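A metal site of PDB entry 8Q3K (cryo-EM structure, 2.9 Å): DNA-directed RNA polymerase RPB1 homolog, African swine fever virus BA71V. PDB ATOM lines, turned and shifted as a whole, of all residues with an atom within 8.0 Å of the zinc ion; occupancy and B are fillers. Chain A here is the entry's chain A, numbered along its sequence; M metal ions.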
ATOM      1  N   ILE A  98       7.427  27.654  12.954  1.00  0.00           N
ATOM      2  CA  ILE A  98       6.188  28.428  12.867  1.00  0.00           C
ATOM      3  C   ILE A  98       4.989  27.491  12.958  1.00  0.00           C
ATOM      4  O   ILE A  98       5.004  26.399  12.383  1.00  0.00           O
ATOM      5  CB  ILE A  98       6.142  29.246  11.563  1.00  0.00           C
ATOM      6  CG1 ILE A  98       7.133  30.421  11.616  1.00  0.00           C
ATOM      7  CG2 ILE A  98       4.736  29.769  11.307  1.00  0.00           C
ATOM      8  CD1 ILE A  98       6.949  31.369  12.800  1.00  0.00           C
ATOM      9  N   CYS A  99       3.951  27.933  13.663  1.00  0.00           N
ATOM     10  CA  CYS A  99       2.700  27.185  13.724  1.00  0.00           C
ATOM     11  C   CYS A  99       2.038  27.176  12.355  1.00  0.00           C
ATOM     12  O   CYS A  99       1.948  28.217  11.690  1.00  0.00           O
ATOM     13  CB  CYS A  99       1.760  27.800  14.765  1.00  0.00           C
ATOM     14  SG  CYS A  99       0.041  27.206  14.725  1.00  0.00           S
ATOM     15  N   LEU A 100       1.581  26.005  11.920  1.00  0.00           N
ATOM     16  CA  LEU A 100       0.922  25.894  10.627  1.00  0.00           C
ATOM     17  C   LEU A 100      -0.492  26.470  10.661  1.00  0.00           C
ATOM     18  O   LEU A 100      -0.922  27.128   9.711  1.00  0.00           O
ATOM     19  CB  LEU A 100       0.894  24.440  10.167  1.00  0.00           C
ATOM     20  CG  LEU A 100       2.205  23.916   9.586  1.00  0.00           C
ATOM     21  CD1 LEU A 100       3.305  23.871  10.631  1.00  0.00           C
ATOM     22  CD2 LEU A 100       2.008  22.543   8.970  1.00  0.00           C
ATOM     23  N   ASN A 101      -1.219  26.230  11.751  1.00  0.00           N
ATOM     24  CA  ASN A 101      -2.607  26.710  11.826  1.00  0.00           C
ATOM     25  C   ASN A 101      -2.664  28.232  11.911  1.00  0.00           C
ATOM     26  O   ASN A 101      -3.507  28.855  11.265  1.00  0.00           O
ATOM     27  CB  ASN A 101      -3.305  26.075  13.024  1.00  0.00           C
ATOM     28  CG  ASN A 101      -4.778  26.415  13.087  1.00  0.00           C
ATOM     29  OD1 ASN A 101      -5.352  26.918  12.116  1.00  0.00           O
ATOM     30  ND2 ASN A 101      -5.400  26.120  14.221  1.00  0.00           N
ATOM     31  N   CYS A 102      -1.789  28.841  12.709  1.00  0.00           N
ATOM     32  CA  CYS A 102      -1.731  30.288  12.862  1.00  0.00           C
ATOM     33  C   CYS A 102      -0.289  30.752  12.773  1.00  0.00           C
ATOM     34  O   CYS A 102       0.659  29.958  12.838  1.00  0.00           O
ATOM     35  CB  CYS A 102      -2.341  30.737  14.191  1.00  0.00           C
ATOM     36  SG  CYS A 102      -1.189  30.667  15.592  1.00  0.00           S
ATOM     37  N   GLY A 103      -0.115  32.065  12.636  1.00  0.00           N
ATOM     38  CA  GLY A 103       1.210  32.633  12.469  1.00  0.00           C
ATOM     39  C   GLY A 103       2.039  32.701  13.735  1.00  0.00           C
ATOM     40  O   GLY A 103       3.232  33.016  13.647  1.00  0.00           O
ATOM     41  N   ALA A 104       1.446  32.436  14.889  1.00  0.00           N
ATOM     42  CA  ALA A 104       2.198  32.524  16.132  1.00  0.00           C
ATOM     43  C   ALA A 104       3.318  31.486  16.146  1.00  0.00           C
ATOM     44  O   ALA A 104       3.132  30.363  15.661  1.00  0.00           O
ATOM     45  CB  ALA A 104       1.279  32.318  17.338  1.00  0.00           C
ATOM     46  N   PRO A 105       4.493  31.825  16.671  1.00  0.00           N
ATOM     47  CA  PRO A 105       5.573  30.838  16.737  1.00  0.00           C
ATOM     48  C   PRO A 105       5.264  29.730  17.733  1.00  0.00           C
ATOM     49  O   PRO A 105       4.555  29.925  18.712  1.00  0.00           O
ATOM     50  CB  PRO A 105       6.782  31.662  17.193  1.00  0.00           C
ATOM     51  CG  PRO A 105       6.194  32.799  17.947  1.00  0.00           C
ATOM     52  CD  PRO A 105       4.890  33.119  17.260  1.00  0.00           C
ATOM     53  N   ILE A 106       5.820  28.547  17.452  1.00  0.00           N
ATOM     54  CA  ILE A 106       5.690  27.408  18.358  1.00  0.00           C
ATOM     55  C   ILE A 106       6.857  27.285  19.311  1.00  0.00           C
ATOM     56  O   ILE A 106       6.942  26.309  20.061  1.00  0.00           O
ATOM     57  CB  ILE A 106       5.516  26.093  17.564  1.00  0.00           C
ATOM     58  CG1 ILE A 106       6.843  25.675  16.917  1.00  0.00           C
ATOM     59  CG2 ILE A 106       4.421  26.236  16.529  1.00  0.00           C
ATOM     60  CD1 ILE A 106       6.761  24.374  16.168  1.00  0.00           C
ATOM     61  N   GLN A 133       2.698  21.953  21.098  1.00  0.00           N
ATOM     62  CA  GLN A 133       1.330  22.380  20.847  1.00  0.00           C
ATOM     63  C   GLN A 133       1.263  23.902  20.901  1.00  0.00           C
ATOM     64  O   GLN A 133       1.785  24.508  21.839  1.00  0.00           O
ATOM     65  CB  GLN A 133       0.372  21.764  21.868  1.00  0.00           C
ATOM     66  CG  GLN A 133      -1.032  22.349  21.848  1.00  0.00           C
ATOM     67  CD  GLN A 133      -2.035  21.476  22.575  1.00  0.00           C
ATOM     68  OE1 GLN A 133      -1.728  20.344  22.950  1.00  0.00           O
ATOM     69  NE2 GLN A 133      -3.234  21.991  22.776  1.00  0.00           N
ATOM     70  N   CYS A 134       0.628  24.504  19.896  1.00  0.00           N
ATOM     71  CA  CYS A 134       0.541  25.946  19.819  1.00  0.00           C
ATOM     72  C   CYS A 134      -0.302  26.493  20.967  1.00  0.00           C
ATOM     73  O   CYS A 134      -1.291  25.883  21.386  1.00  0.00           O
ATOM     74  CB  CYS A 134      -0.051  26.366  18.471  1.00  0.00           C
ATOM     75  SG  CYS A 134      -0.625  28.076  18.367  1.00  0.00           S
ATOM     76  N   TYR A 135       0.112  27.649  21.503  1.00  0.00           N
ATOM     77  CA  TYR A 135      -0.616  28.240  22.616  1.00  0.00           C
ATOM     78  C   TYR A 135      -2.007  28.682  22.199  1.00  0.00           C
ATOM     79  O   TYR A 135      -2.988  28.444  22.914  1.00  0.00           O
ATOM     80  CB  TYR A 135       0.173  29.408  23.201  1.00  0.00           C
ATOM     81  CG  TYR A 135      -0.314  29.902  24.549  1.00  0.00           C
ATOM     82  CD1 TYR A 135      -1.252  29.184  25.288  1.00  0.00           C
ATOM     83  CD2 TYR A 135       0.164  31.086  25.097  1.00  0.00           C
ATOM     84  CE1 TYR A 135      -1.700  29.635  26.522  1.00  0.00           C
ATOM     85  CE2 TYR A 135      -0.262  31.538  26.327  1.00  0.00           C
ATOM     86  CZ  TYR A 135      -1.196  30.816  27.030  1.00  0.00           C
ATOM     87  OH  TYR A 135      -1.631  31.263  28.260  1.00  0.00           O
ATOM     88  N   VAL A 136      -2.124  29.341  21.049  1.00  0.00           N
ATOM     89  CA  VAL A 136      -3.424  29.828  20.591  1.00  0.00           C
ATOM     90  C   VAL A 136      -4.147  28.823  19.701  1.00  0.00           C
ATOM     91  O   VAL A 136      -5.355  28.956  19.502  1.00  0.00           O
ATOM     92  CB  VAL A 136      -3.283  31.173  19.852  1.00  0.00           C
ATOM     93  CG1 VAL A 136      -2.395  32.130  20.647  1.00  0.00           C
ATOM     94  CG2 VAL A 136      -2.720  30.974  18.454  1.00  0.00           C
ATOM     95  N   CYS A 137      -3.440  27.827  19.177  1.00  0.00           N
ATOM     96  CA  CYS A 137      -4.040  26.746  18.408  1.00  0.00           C
ATOM     97  C   CYS A 137      -3.840  25.437  19.168  1.00  0.00           C
ATOM     98  O   CYS A 137      -2.721  25.111  19.563  1.00  0.00           O
ATOM     99  CB  CYS A 137      -3.416  26.624  17.022  1.00  0.00           C
ATOM    100  SG  CYS A 137      -3.649  28.046  15.953  1.00  0.00           S
ATOM    101  N   LYS A 138      -4.931  24.698  19.349  1.00  0.00           N
ATOM    102  CA  LYS A 138      -4.805  23.373  19.948  1.00  0.00           C
ATOM    103  C   LYS A 138      -4.066  22.395  19.049  1.00  0.00           C
ATOM    104  O   LYS A 138      -3.698  21.312  19.512  1.00  0.00           O
ATOM    105  CB  LYS A 138      -6.188  22.814  20.295  1.00  0.00           C
ATOM    106  CG  LYS A 138      -6.871  23.554  21.433  1.00  0.00           C
ATOM    107  CD  LYS A 138      -8.134  22.839  21.888  1.00  0.00           C
ATOM    108  CE  LYS A 138      -8.735  23.498  23.120  1.00  0.00           C
ATOM    109  NZ  LYS A 138      -9.960  22.796  23.586  1.00  0.00           N
ATOM    110  N   ALA A 139      -3.845  22.758  17.784  1.00  0.00           N
ATOM    111  CA  ALA A 139      -3.118  21.890  16.880  1.00  0.00           C
ATOM    112  C   ALA A 139      -1.710  21.625  17.384  1.00  0.00           C
ATOM    113  O   ALA A 139      -1.046  22.516  17.913  1.00  0.00           O
ATOM    114  CB  ALA A 139      -3.072  22.517  15.487  1.00  0.00           C
ATOM    115  N   ARG A 176       0.293  34.271   7.308  1.00  0.00           N
ATOM    116  CA  ARG A 176      -0.229  34.640   8.619  1.00  0.00           C
ATOM    117  C   ARG A 176       0.863  35.008   9.615  1.00  0.00           C
ATOM    118  O   ARG A 176       0.548  35.543  10.684  1.00  0.00           O
ATOM    119  CB  ARG A 176      -1.077  33.502   9.200  1.00  0.00           C
ATOM    120  CG  ARG A 176      -1.741  32.613   8.152  1.00  0.00           C
ATOM    121  CD  ARG A 176      -2.736  31.668   8.789  1.00  0.00           C
ATOM    122  NE  ARG A 176      -3.115  30.587   7.870  1.00  0.00           N
ATOM    123  CZ  ARG A 176      -2.479  29.428   7.785  1.00  0.00           C
ATOM    124  NH1 ARG A 176      -1.433  29.143   8.545  1.00  0.00           N
ATOM    125  NH2 ARG A 176      -2.907  28.525   6.909  1.00  0.00           N
HETATM  126 ZN    ZN M   1      -1.351  28.418  16.167  1.00  0.00          ZN
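CG2 of Val 136 touches the zinc ion, at 3.7 Å.
Five residues have an atom within 4 Å of the zinc ion: Cys 99, Cys 102, Cys 134, Val 136 and Cys 137.
The nearest printed residue that does not touch the zinc ion is Asn 101 (4.4 Å).
The zinc ion is bound by the side-chain sulfur of Cys 102 (2.3 Å), the side-chain sulfur of Cys 137 (2.3 Å), the side-chain sulfur of Cys 134 (2.3 Å) and the side-chain sulfur of Cys 99 (2.3 Å).
N of Ala 104 sits close to SG of Cys 102 (3.3 Å).
The side-chain sulfur (SG) of Cys 137 lies close to the side-chain amide nitrogen (ND2) of Asn 101, at 3.1 Å.
The side-chain sulfur (SG) of Cys 134 sits close to the backbone NH (N) of Val 136 (3.3 Å).
The backbone carbonyl oxygen of Ala 139 lies within hydrogen-bond range of the backbone NH of Cys 134.
SG of Cys 99 lies close to N of Asn 101, 3.4 Å away.
O of Ala 104 lies close to N of Cys 99 (3.3 Å).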
